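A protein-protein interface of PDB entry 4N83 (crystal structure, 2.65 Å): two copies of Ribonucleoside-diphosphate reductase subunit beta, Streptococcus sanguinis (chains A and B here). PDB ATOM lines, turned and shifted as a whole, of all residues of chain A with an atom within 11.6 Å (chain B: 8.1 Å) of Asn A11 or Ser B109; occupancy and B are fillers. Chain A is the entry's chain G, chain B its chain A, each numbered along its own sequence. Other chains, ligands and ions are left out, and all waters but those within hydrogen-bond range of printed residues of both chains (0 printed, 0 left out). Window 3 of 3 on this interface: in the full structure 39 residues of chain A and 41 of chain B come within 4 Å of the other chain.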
ATOM      1  N   ALA A   7       4.037  -0.318  13.330  1.00  0.00           N
ATOM      2  CA  ALA A   7       3.109  -1.199  12.625  1.00  0.00           C
ATOM      3  C   ALA A   7       2.739  -0.612  11.266  1.00  0.00           C
ATOM      4  O   ALA A   7       2.639   0.609  11.117  1.00  0.00           O
ATOM      5  CB  ALA A   7       1.857  -1.425  13.460  1.00  0.00           C
ATOM      6  N   ILE A   8       2.538  -1.486  10.282  1.00  0.00           N
ATOM      7  CA  ILE A   8       2.148  -1.068   8.935  1.00  0.00           C
ATOM      8  C   ILE A   8       0.640  -0.809   8.886  1.00  0.00           C
ATOM      9  O   ILE A   8      -0.150  -1.592   9.419  1.00  0.00           O
ATOM     10  CB  ILE A   8       2.566  -2.109   7.867  1.00  0.00           C
ATOM     11  CG1 ILE A   8       2.482  -1.500   6.464  1.00  0.00           C
ATOM     12  CG2 ILE A   8       1.720  -3.375   7.951  1.00  0.00           C
ATOM     13  CD1 ILE A   8       3.120  -2.357   5.392  1.00  0.00           C
ATOM     14  N   ASN A   9       0.253   0.294   8.251  1.00  0.00           N
ATOM     15  CA  ASN A   9      -1.142   0.728   8.214  1.00  0.00           C
ATOM     16  C   ASN A   9      -1.608   0.975   6.783  1.00  0.00           C
ATOM     17  O   ASN A   9      -1.096   1.868   6.108  1.00  0.00           O
ATOM     18  CB  ASN A   9      -1.309   2.004   9.046  1.00  0.00           C
ATOM     19  CG  ASN A   9      -2.766   2.378   9.275  1.00  0.00           C
ATOM     20  OD1 ASN A   9      -3.681   1.749   8.739  1.00  0.00           O
ATOM     21  ND2 ASN A   9      -2.987   3.410  10.081  1.00  0.00           N
ATOM     22  N   TRP A  10      -2.586   0.190   6.335  1.00  0.00           N
ATOM     23  CA  TRP A  10      -3.116   0.303   4.973  1.00  0.00           C
ATOM     24  C   TRP A  10      -4.366   1.190   4.898  1.00  0.00           C
ATOM     25  O   TRP A  10      -5.065   1.193   3.884  1.00  0.00           O
ATOM     26  CB  TRP A  10      -3.403  -1.089   4.403  1.00  0.00           C
ATOM     27  CG  TRP A  10      -2.184  -1.965   4.349  1.00  0.00           C
ATOM     28  CD1 TRP A  10      -1.646  -2.685   5.377  1.00  0.00           C
ATOM     29  CD2 TRP A  10      -1.349  -2.206   3.211  1.00  0.00           C
ATOM     30  NE1 TRP A  10      -0.529  -3.363   4.948  1.00  0.00           N
ATOM     31  CE2 TRP A  10      -0.323  -3.087   3.623  1.00  0.00           C
ATOM     32  CE3 TRP A  10      -1.366  -1.764   1.880  1.00  0.00           C
ATOM     33  CZ2 TRP A  10       0.674  -3.536   2.753  1.00  0.00           C
ATOM     34  CZ3 TRP A  10      -0.372  -2.212   1.015  1.00  0.00           C
ATOM     35  CH2 TRP A  10       0.634  -3.090   1.457  1.00  0.00           C
ATOM     36  N   ASN A  11      -4.644   1.926   5.975  1.00  0.00           N
ATOM     37  CA  ASN A  11      -5.652   2.993   5.970  1.00  0.00           C
ATOM     38  C   ASN A  11      -5.003   4.377   5.868  1.00  0.00           C
ATOM     39  O   ASN A  11      -5.587   5.295   5.290  1.00  0.00           O
ATOM     40  CB  ASN A  11      -6.527   2.914   7.224  1.00  0.00           C
ATOM     41  CG  ASN A  11      -7.484   1.736   7.193  1.00  0.00           C
ATOM     42  OD1 ASN A  11      -8.382   1.681   6.355  1.00  0.00           O
ATOM     43  ND2 ASN A  11      -7.302   0.791   8.111  1.00  0.00           N
ATOM     44  N   ALA A  12      -3.805   4.516   6.437  1.00  0.00           N
ATOM     45  CA  ALA A  12      -3.018   5.743   6.331  1.00  0.00           C
ATOM     46  C   ALA A  12      -1.981   5.606   5.218  1.00  0.00           C
ATOM     47  O   ALA A  12      -0.791   5.416   5.481  1.00  0.00           O
ATOM     48  CB  ALA A  12      -2.341   6.054   7.660  1.00  0.00           C
ATOM     49  N   ILE A  13      -2.445   5.705   3.972  1.00  0.00           N
ATOM     50  CA  ILE A  13      -1.578   5.560   2.798  1.00  0.00           C
ATOM     51  C   ILE A  13      -0.644   6.765   2.668  1.00  0.00           C
ATOM     52  O   ILE A  13      -1.079   7.913   2.775  1.00  0.00           O
ATOM     53  CB  ILE A  13      -2.398   5.376   1.490  1.00  0.00           C
ATOM     54  CG1 ILE A  13      -2.942   3.945   1.388  1.00  0.00           C
ATOM     55  CG2 ILE A  13      -1.550   5.659   0.256  1.00  0.00           C
ATOM     56  CD1 ILE A  13      -4.102   3.650   2.311  1.00  0.00           C
ATOM     57  N   GLU A  14       0.637   6.486   2.431  1.00  0.00           N
ATOM     58  CA  GLU A  14       1.653   7.521   2.236  1.00  0.00           C
ATOM     59  C   GLU A  14       1.807   7.844   0.752  1.00  0.00           C
ATOM     60  O   GLU A  14       1.936   9.010   0.376  1.00  0.00           O
ATOM     61  CB  GLU A  14       2.994   7.062   2.815  1.00  0.00           C
ATOM     62  CG  GLU A  14       2.976   6.846   4.321  1.00  0.00           C
ATOM     63  CD  GLU A  14       4.262   6.230   4.842  1.00  0.00           C
ATOM     64  OE1 GLU A  14       4.183   5.218   5.568  1.00  0.00           O
ATOM     65  OE2 GLU A  14       5.351   6.755   4.523  1.00  0.00           O
ATOM     66  N   ASP A  15       1.799   6.802  -0.079  1.00  0.00           N
ATOM     67  CA  ASP A  15       1.864   6.944  -1.533  1.00  0.00           C
ATOM     68  C   ASP A  15       0.727   6.137  -2.166  1.00  0.00           C
ATOM     69  O   ASP A  15       0.610   4.934  -1.930  1.00  0.00           O
ATOM     70  CB  ASP A  15       3.222   6.450  -2.043  1.00  0.00           C
ATOM     71  CG  ASP A  15       3.585   7.022  -3.402  1.00  0.00           C
ATOM     72  OD1 ASP A  15       2.672   7.327  -4.200  1.00  0.00           O
ATOM     73  OD2 ASP A  15       4.796   7.161  -3.674  1.00  0.00           O
ATOM     74  N   VAL A  16      -0.105   6.804  -2.966  1.00  0.00           N
ATOM     75  CA  VAL A  16      -1.301   6.173  -3.554  1.00  0.00           C
ATOM     76  C   VAL A  16      -0.984   5.054  -4.552  1.00  0.00           C
ATOM     77  O   VAL A  16      -1.808   4.159  -4.757  1.00  0.00           O
ATOM     78  CB  VAL A  16      -2.242   7.206  -4.232  1.00  0.00           C
ATOM     79  CG1 VAL A  16      -2.719   8.243  -3.221  1.00  0.00           C
ATOM     80  CG2 VAL A  16      -1.577   7.875  -5.432  1.00  0.00           C
ATOM     81  N   ASP A  18       1.380   2.780  -4.159  1.00  0.00           N
ATOM     82  CA  ASP A  18       1.656   1.566  -3.374  1.00  0.00           C
ATOM     83  C   ASP A  18       0.417   0.688  -3.200  1.00  0.00           C
ATOM     84  O   ASP A  18       0.509  -0.540  -3.241  1.00  0.00           O
ATOM     85  CB  ASP A  18       2.212   1.924  -1.988  1.00  0.00           C
ATOM     86  CG  ASP A  18       3.566   2.609  -2.051  1.00  0.00           C
ATOM     87  OD1 ASP A  18       4.216   2.581  -3.117  1.00  0.00           O
ATOM     88  OD2 ASP A  18       3.980   3.181  -1.022  1.00  0.00           O
ATOM     89  N   LYS A  19      -0.733   1.324  -2.993  1.00  0.00           N
ATOM     90  CA  LYS A  19      -2.007   0.619  -2.864  1.00  0.00           C
ATOM     91  C   LYS A  19      -2.414  -0.023  -4.191  1.00  0.00           C
ATOM     92  O   LYS A  19      -2.779  -1.199  -4.230  1.00  0.00           O
ATOM     93  CB  LYS A  19      -3.103   1.586  -2.397  1.00  0.00           C
ATOM     94  CG  LYS A  19      -4.492   0.968  -2.246  1.00  0.00           C
ATOM     95  CD  LYS A  19      -5.595   2.018  -2.159  1.00  0.00           C
ATOM     96  CE  LYS A  19      -5.799   2.775  -3.467  1.00  0.00           C
ATOM     97  NZ  LYS A  19      -6.070   1.889  -4.635  1.00  0.00           N
ATOM     98  N   SER A  20      -2.350   0.755  -5.270  1.00  0.00           N
ATOM     99  CA  SER A  20      -2.806   0.300  -6.586  1.00  0.00           C
ATOM    100  C   SER A  20      -1.925  -0.807  -7.174  1.00  0.00           C
ATOM    101  O   SER A  20      -2.426  -1.693  -7.871  1.00  0.00           O
ATOM    102  CB  SER A  20      -2.880   1.478  -7.564  1.00  0.00           C
ATOM    103  OG  SER A  20      -1.596   2.014  -7.820  1.00  0.00           O
ATOM    104  N   TRP A  22       0.003  -3.028  -5.368  1.00  0.00           N
ATOM    105  CA  TRP A  22      -0.299  -4.223  -4.579  1.00  0.00           C
ATOM    106  C   TRP A  22      -1.576  -4.874  -5.104  1.00  0.00           C
ATOM    107  O   TRP A  22      -1.604  -6.074  -5.376  1.00  0.00           O
ATOM    108  CB  TRP A  22      -0.460  -3.861  -3.097  1.00  0.00           C
ATOM    109  CG  TRP A  22      -0.947  -4.993  -2.232  1.00  0.00           C
ATOM    110  CD1 TRP A  22      -2.246  -5.313  -1.959  1.00  0.00           C
ATOM    111  CD2 TRP A  22      -0.143  -5.945  -1.523  1.00  0.00           C
ATOM    112  NE1 TRP A  22      -2.301  -6.406  -1.130  1.00  0.00           N
ATOM    113  CE2 TRP A  22      -1.026  -6.812  -0.843  1.00  0.00           C
ATOM    114  CE3 TRP A  22       1.237  -6.150  -1.395  1.00  0.00           C
ATOM    115  CZ2 TRP A  22      -0.574  -7.871  -0.050  1.00  0.00           C
ATOM    116  CZ3 TRP A  22       1.684  -7.202  -0.603  1.00  0.00           C
ATOM    117  CH2 TRP A  22       0.779  -8.047   0.058  1.00  0.00           C
ATOM    118  N   GLU A  23      -2.623  -4.064  -5.256  1.00  0.00           N
ATOM    119  CA  GLU A  23      -3.908  -4.531  -5.788  1.00  0.00           C
ATOM    120  C   GLU A  23      -3.814  -5.064  -7.220  1.00  0.00           C
ATOM    121  O   GLU A  23      -4.686  -5.812  -7.654  1.00  0.00           O
ATOM    122  CB  GLU A  23      -4.953  -3.410  -5.727  1.00  0.00           C
ATOM    123  CG  GLU A  23      -5.470  -3.118  -4.325  1.00  0.00           C
ATOM    124  CD  GLU A  23      -6.490  -1.992  -4.285  1.00  0.00           C
ATOM    125  OE1 GLU A  23      -6.594  -1.230  -5.270  1.00  0.00           O
ATOM    126  OE2 GLU A  23      -7.192  -1.867  -3.260  1.00  0.00           O
ATOM    127  N   THR A  83       8.262   4.176   1.738  1.00  0.00           N
ATOM    128  CA  THR A  83       7.135   3.916   2.641  1.00  0.00           C
ATOM    129  C   THR A  83       7.181   2.486   3.170  1.00  0.00           C
ATOM    130  O   THR A  83       7.917   1.651   2.650  1.00  0.00           O
ATOM    131  CB  THR A  83       5.777   4.134   1.937  1.00  0.00           C
ATOM    132  OG1 THR A  83       5.561   3.101   0.967  1.00  0.00           O
ATOM    133  CG2 THR A  83       5.729   5.495   1.246  1.00  0.00           C
ATOM    134  N   ALA A  84       6.384   2.208   4.198  1.00  0.00           N
ATOM    135  CA  ALA A  84       6.286   0.859   4.763  1.00  0.00           C
ATOM    136  C   ALA A  84       5.509  -0.090   3.842  1.00  0.00           C
ATOM    137  O   ALA A  84       5.711  -1.307   3.881  1.00  0.00           O
ATOM    138  CB  ALA A  84       5.637   0.910   6.139  1.00  0.00           C
ATOM    139  N   HIS A  85       4.625   0.474   3.019  1.00  0.00           N
ATOM    140  CA  HIS A  85       3.836  -0.306   2.059  1.00  0.00           C
ATOM    141  C   HIS A  85       4.711  -0.803   0.913  1.00  0.00           C
ATOM    142  O   HIS A  85       4.528  -1.916   0.427  1.00  0.00           O
ATOM    143  CB  HIS A  85       2.686   0.527   1.479  1.00  0.00           C
ATOM    144  CG  HIS A  85       1.919   1.306   2.501  1.00  0.00           C
ATOM    145  ND1 HIS A  85       1.970   2.681   2.577  1.00  0.00           N
ATOM    146  CD2 HIS A  85       1.090   0.904   3.494  1.00  0.00           C
ATOM    147  CE1 HIS A  85       1.202   3.094   3.570  1.00  0.00           C
ATOM    148  NE2 HIS A  85       0.657   2.036   4.141  1.00  0.00           N
ATOM    149  N   LEU B  37     -16.475  -9.002   4.562  1.00  0.00           N
ATOM    150  CA  LEU B  37     -16.464  -8.596   5.970  1.00  0.00           C
ATOM    151  C   LEU B  37     -17.711  -7.804   6.380  1.00  0.00           C
ATOM    152  O   LEU B  37     -18.011  -7.693   7.571  1.00  0.00           O
ATOM    153  CB  LEU B  37     -15.203  -7.778   6.270  1.00  0.00           C
ATOM    154  CG  LEU B  37     -13.891  -8.568   6.183  1.00  0.00           C
ATOM    155  CD1 LEU B  37     -12.711  -7.649   5.907  1.00  0.00           C
ATOM    156  CD2 LEU B  37     -13.662  -9.375   7.453  1.00  0.00           C
ATOM    157  N   LEU B  41     -21.093  -7.141  10.199  1.00  0.00           N
ATOM    158  CA  LEU B  41     -21.506  -5.904  10.865  1.00  0.00           C
ATOM    159  C   LEU B  41     -22.782  -6.091  11.689  1.00  0.00           C
ATOM    160  O   LEU B  41     -23.068  -5.287  12.576  1.00  0.00           O
ATOM    161  CB  LEU B  41     -21.706  -4.777   9.845  1.00  0.00           C
ATOM    162  CG  LEU B  41     -20.423  -4.165   9.275  1.00  0.00           C
ATOM    163  CD1 LEU B  41     -20.726  -3.297   8.062  1.00  0.00           C
ATOM    164  CD2 LEU B  41     -19.688  -3.363  10.340  1.00  0.00           C
ATOM    165  N   LYS B 102      -1.558  -6.933   6.246  1.00  0.00           N
ATOM    166  CA  LYS B 102      -2.596  -6.152   5.567  1.00  0.00           C
ATOM    167  C   LYS B 102      -4.005  -6.569   5.990  1.00  0.00           C
ATOM    168  O   LYS B 102      -4.861  -5.714   6.217  1.00  0.00           O
ATOM    169  CB  LYS B 102      -2.458  -6.264   4.041  1.00  0.00           C
ATOM    170  CG  LYS B 102      -3.578  -5.574   3.271  1.00  0.00           C
ATOM    171  CD  LYS B 102      -3.325  -5.562   1.775  1.00  0.00           C
ATOM    172  CE  LYS B 102      -4.586  -5.195   1.006  1.00  0.00           C
ATOM    173  NZ  LYS B 102      -5.117  -3.856   1.383  1.00  0.00           N
ATOM    174  N   SER B 103      -4.237  -7.877   6.096  1.00  0.00           N
ATOM    175  CA  SER B 103      -5.569  -8.418   6.398  1.00  0.00           C
ATOM    176  C   SER B 103      -6.247  -7.755   7.605  1.00  0.00           C
ATOM    177  O   SER B 103      -7.469  -7.599   7.621  1.00  0.00           O
ATOM    178  CB  SER B 103      -5.496  -9.934   6.608  1.00  0.00           C
ATOM    179  OG  SER B 103      -4.550 -10.271   7.606  1.00  0.00           O
ATOM    180  N   TYR B 104      -5.454  -7.368   8.602  1.00  0.00           N
ATOM    181  CA  TYR B 104      -5.976  -6.672   9.781  1.00  0.00           C
ATOM    182  C   TYR B 104      -6.588  -5.318   9.419  1.00  0.00           C
ATOM    183  O   TYR B 104      -7.616  -4.933   9.977  1.00  0.00           O
ATOM    184  CB  TYR B 104      -4.877  -6.462  10.824  1.00  0.00           C
ATOM    185  CG  TYR B 104      -4.212  -7.733  11.302  1.00  0.00           C
ATOM    186  CD1 TYR B 104      -4.947  -8.729  11.938  1.00  0.00           C
ATOM    187  CD2 TYR B 104      -2.846  -7.932  11.133  1.00  0.00           C
ATOM    188  CE1 TYR B 104      -4.339  -9.893  12.383  1.00  0.00           C
ATOM    189  CE2 TYR B 104      -2.229  -9.089  11.575  1.00  0.00           C
ATOM    190  CZ  TYR B 104      -2.978 -10.069  12.199  1.00  0.00           C
ATOM    191  OH  TYR B 104      -2.368 -11.222  12.640  1.00  0.00           O
ATOM    192  N   SER B 105      -5.950  -4.603   8.493  1.00  0.00           N
ATOM    193  CA  SER B 105      -6.438  -3.293   8.046  1.00  0.00           C
ATOM    194  C   SER B 105      -7.816  -3.382   7.382  1.00  0.00           C
ATOM    195  O   SER B 105      -8.627  -2.461   7.506  1.00  0.00           O
ATOM    196  CB  SER B 105      -5.437  -2.637   7.087  1.00  0.00           C
ATOM    197  OG  SER B 105      -4.154  -2.521   7.679  1.00  0.00           O
ATOM    198  N   SER B 106      -8.072  -4.489   6.682  1.00  0.00           N
ATOM    199  CA  SER B 106      -9.377  -4.740   6.061  1.00  0.00           C
ATOM    200  C   SER B 106     -10.463  -5.007   7.102  1.00  0.00           C
ATOM    201  O   SER B 106     -11.624  -4.651   6.896  1.00  0.00           O
ATOM    202  CB  SER B 106      -9.292  -5.924   5.097  1.00  0.00           C
ATOM    203  OG  SER B 106      -8.344  -5.675   4.078  1.00  0.00           O
ATOM    204  N   ILE B 107     -10.081  -5.639   8.211  1.00  0.00           N
ATOM    205  CA  ILE B 107     -10.997  -5.873   9.327  1.00  0.00           C
ATOM    206  C   ILE B 107     -11.386  -4.545   9.967  1.00  0.00           C
ATOM    207  O   ILE B 107     -12.562  -4.303  10.239  1.00  0.00           O
ATOM    208  CB  ILE B 107     -10.371  -6.789  10.406  1.00  0.00           C
ATOM    209  CG1 ILE B 107     -10.133  -8.196   9.844  1.00  0.00           C
ATOM    210  CG2 ILE B 107     -11.264  -6.862  11.641  1.00  0.00           C
ATOM    211  CD1 ILE B 107      -9.213  -9.048  10.694  1.00  0.00           C
ATOM    212  N   PHE B 108     -10.392  -3.689  10.195  1.00  0.00           N
ATOM    213  CA  PHE B 108     -10.620  -2.383  10.815  1.00  0.00           C
ATOM    214  C   PHE B 108     -11.476  -1.471   9.932  1.00  0.00           C
ATOM    215  O   PHE B 108     -12.319  -0.728  10.439  1.00  0.00           O
ATOM    216  CB  PHE B 108      -9.293  -1.675  11.131  1.00  0.00           C
ATOM    217  CG  PHE B 108      -8.380  -2.441  12.058  1.00  0.00           C
ATOM    218  CD1 PHE B 108      -8.867  -3.038  13.216  1.00  0.00           C
ATOM    219  CD2 PHE B 108      -7.019  -2.532  11.785  1.00  0.00           C
ATOM    220  CE1 PHE B 108      -8.020  -3.732  14.066  1.00  0.00           C
ATOM    221  CE2 PHE B 108      -6.169  -3.223  12.632  1.00  0.00           C
ATOM    222  CZ  PHE B 108      -6.669  -3.823  13.775  1.00  0.00           C
ATOM    223  N   SER B 109     -11.256  -1.529   8.621  1.00  0.00           N
ATOM    224  CA  SER B 109     -11.968  -0.664   7.676  1.00  0.00           C
ATOM    225  C   SER B 109     -13.478  -0.892   7.693  1.00  0.00           C
ATOM    226  O   SER B 109     -14.252   0.066   7.697  1.00  0.00           O
ATOM    227  CB  SER B 109     -11.435  -0.867   6.257  1.00  0.00           C
ATOM    228  OG  SER B 109     -10.067  -0.513   6.175  1.00  0.00           O
ATOM    229  N   THR B 110     -13.888  -2.159   7.706  1.00  0.00           N
ATOM    230  CA  THR B 110     -15.307  -2.513   7.690  1.00  0.00           C
ATOM    231  C   THR B 110     -15.957  -2.251   9.048  1.00  0.00           C
ATOM    232  O   THR B 110     -16.967  -1.552   9.132  1.00  0.00           O
ATOM    233  CB  THR B 110     -15.519  -3.994   7.310  1.00  0.00           C
ATOM    234  OG1 THR B 110     -14.657  -4.345   6.222  1.00  0.00           O
ATOM    235  CG2 THR B 110     -16.970  -4.245   6.908  1.00  0.00           C
ATOM    236  N   LEU B 111     -15.368  -2.811  10.102  1.00  0.00           N
ATOM    237  CA  LEU B 111     -15.925  -2.714  11.454  1.00  0.00           C
ATOM    238  C   LEU B 111     -15.844  -1.298  12.019  1.00  0.00           C
ATOM    239  O   LEU B 111     -16.856  -0.735  12.439  1.00  0.00           O
ATOM    240  CB  LEU B 111     -15.212  -3.683  12.410  1.00  0.00           C
ATOM    241  CG  LEU B 111     -15.672  -5.145  12.413  1.00  0.00           C
ATOM    242  CD1 LEU B 111     -15.593  -5.784  11.033  1.00  0.00           C
ATOM    243  CD2 LEU B 111     -14.854  -5.941  13.421  1.00  0.00           C
ATOM    244  N   ASN B 112     -14.639  -0.731  12.017  1.00  0.00           N
ATOM    245  CA  ASN B 112     -14.369   0.542  12.693  1.00  0.00           C
ATOM    246  C   ASN B 112     -14.384   1.751  11.758  1.00  0.00           C
ATOM    247  O   ASN B 112     -14.391   1.609  10.533  1.00  0.00           O
ATOM    248  CB  ASN B 112     -13.022   0.475  13.421  1.00  0.00           C
ATOM    249  CG  ASN B 112     -12.898  -0.749  14.311  1.00  0.00           C
ATOM    250  OD1 ASN B 112     -13.876  -1.196  14.911  1.00  0.00           O
ATOM    251  ND2 ASN B 112     -11.692  -1.300  14.401  1.00  0.00           N
ATOM    252  N   THR B 113     -14.388   2.938  12.363  1.00  0.00           N
ATOM    253  CA  THR B 113     -14.394   4.210  11.636  1.00  0.00           C
ATOM    254  C   THR B 113     -12.982   4.788  11.505  1.00  0.00           C
ATOM    255  O   THR B 113     -12.044   4.307  12.144  1.00  0.00           O
ATOM    256  CB  THR B 113     -15.292   5.246  12.343  1.00  0.00           C
ATOM    257  OG1 THR B 113     -14.804   5.484  13.670  1.00  0.00           O
ATOM    258  CG2 THR B 113     -16.730   4.750  12.415  1.00  0.00           C
ATOM    259  N   LYS B 114     -12.850   5.829  10.684  1.00  0.00           N
ATOM    260  CA  LYS B 114     -11.556   6.457  10.378  1.00  0.00           C
ATOM    261  C   LYS B 114     -10.736   6.786  11.627  1.00  0.00           C
ATOM    262  O   LYS B 114      -9.577   6.382  11.738  1.00  0.00           O
ATOM    263  CB  LYS B 114     -11.776   7.731   9.551  1.00  0.00           C
ATOM    264  CG  LYS B 114     -10.505   8.444   9.110  1.00  0.00           C
ATOM    265  CD  LYS B 114     -10.830   9.640   8.229  1.00  0.00           C
ATOM    266  CE  LYS B 114      -9.623  10.544   8.030  1.00  0.00           C
ATOM    267  NZ  LYS B 114      -8.545   9.895   7.235  1.00  0.00           N
ATOM    268  N   ILE B 117      -9.663   3.843  13.986  1.00  0.00           N
ATOM    269  CA  ILE B 117      -8.486   3.122  13.499  1.00  0.00           C
ATOM    270  C   ILE B 117      -7.211   3.845  13.936  1.00  0.00           C
ATOM    271  O   ILE B 117      -6.241   3.206  14.347  1.00  0.00           O
ATOM    272  CB  ILE B 117      -8.506   2.958  11.962  1.00  0.00           C
ATOM    273  CG1 ILE B 117      -9.744   2.164  11.524  1.00  0.00           C
ATOM    274  CG2 ILE B 117      -7.249   2.237  11.485  1.00  0.00           C
ATOM    275  CD1 ILE B 117     -10.138   2.379  10.079  1.00  0.00           C
ATOM    276  N   ASP B 118      -7.220   5.175  13.852  1.00  0.00           N
ATOM    277  CA  ASP B 118      -6.111   5.996  14.348  1.00  0.00           C
ATOM    278  C   ASP B 118      -5.854   5.746  15.836  1.00  0.00           C
ATOM    279  O   ASP B 118      -4.703   5.713  16.274  1.00  0.00           O
ATOM    280  CB  ASP B 118      -6.394   7.487  14.126  1.00  0.00           C
ATOM    281  CG  ASP B 118      -6.343   7.885  12.663  1.00  0.00           C
ATOM    282  OD1 ASP B 118      -5.354   7.542  11.984  1.00  0.00           O
ATOM    283  OD2 ASP B 118      -7.288   8.555  12.194  1.00  0.00           O
ATOM    284  N   PHE B 121      -4.112   2.044  16.255  1.00  0.00           N
ATOM    285  CA  PHE B 121      -2.708   2.062  15.820  1.00  0.00           C
ATOM    286  C   PHE B 121      -1.818   2.900  16.741  1.00  0.00           C
ATOM    287  O   PHE B 121      -0.656   2.556  16.962  1.00  0.00           O
ATOM    288  CB  PHE B 121      -2.582   2.559  14.369  1.00  0.00           C
ATOM    289  CG  PHE B 121      -2.818   1.487  13.339  1.00  0.00           C
ATOM    290  CD1 PHE B 121      -1.861   0.506  13.111  1.00  0.00           C
ATOM    291  CD2 PHE B 121      -3.991   1.457  12.596  1.00  0.00           C
ATOM    292  CE1 PHE B 121      -2.072  -0.485  12.166  1.00  0.00           C
ATOM    293  CE2 PHE B 121      -4.208   0.468  11.648  1.00  0.00           C
ATOM    294  CZ  PHE B 121      -3.246  -0.504  11.432  1.00  0.00           C
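The backbone NH (N) of Trp A10 sits close to the side-chain hydroxyl (OG) of Ser B105 (3.4 Å). OG of Ser B109 is in hydrogen-bond range of OD1 of Asn A11 (2.8 Å).
The backbone carbonyl oxygen (O) of Ser B105 sits at hydrogen-bond distance from the side-chain hydroxyl (OG) of Ser B109, 2.8 Å away. N of Asn A11 is in hydrogen-bond range of OD1 of Asn A9 (2.9 Å). A ring nitrogen (NE2) of His A85 lies within hydrogen-bond range of the backbone carbonyl oxygen (O) of Asn A9.
Ile A8 touches Phe B121. Phe B121 touches Asn A9 (CE2 to OD1, 3.2 Å). CA of Lys B102 touches NE1 of Trp A10, at 3.5 Å. Ser B105 touches Asn A11 (O to ND2, 3.6 Å). Asn A11 touches Ile B117. CD of Lys B102 touches NE1 of Trp A22, 3.2 Å away.
Printed residues of chain B within 4 Å of Asn A11: Ser B105, Ser B109 and Ile B117. Ser B109 touches just one residue of chain A: Asn A11. Ser B105 touches just these residues of chain A: Trp A10 (3.4 Å) and Asn A11 (3.6 Å). No residue of chain A comes within 4 Å of Ser B106. No residue of chain A comes within 4 Å of Phe B108. No residue of chain A comes within 4 Å of Thr B110. No residue of chain A comes within 4 Å of Asn B112. Lys B114 touches none of the printed residues of chain A. Of the printed residues of chain B, Ile A8 touches Phe B121 (3.5 Å). Of the printed residues of chain A, Phe B121 touches Ile A8 (3.5 Å) and Asn A9 (3.2 Å). Of the printed residues of chain B, Asn A9 touches Phe B121 (3.2 Å). Printed residues of chain B within 4 Å of Trp A10: Lys B102 (3.5 Å) and Ser B105 (3.4 Å). Of the printed residues of chain B, Trp A22 touches Lys B102. His A85 touches none of the printed residues of chain B. Thr B113 touches none of the printed residues of chain A. The nearest residue of chain B that does not touch Asn A11 is Phe B108 (4.4 Å). The nearest residue of chain A that does not touch Ser B109 is Trp A10 (5.8 Å).
Of the 18 printed residues of chain B, 5 touch a printed residue of chain A. Of the 18 printed residues of chain A, 5 touch a printed residue of chain B. Among the printed residues, no Asp or Glu carboxylate lies within 4 Å of a Lys or Arg side-chain nitrogen of the other chain.
No position is printed for both chains.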
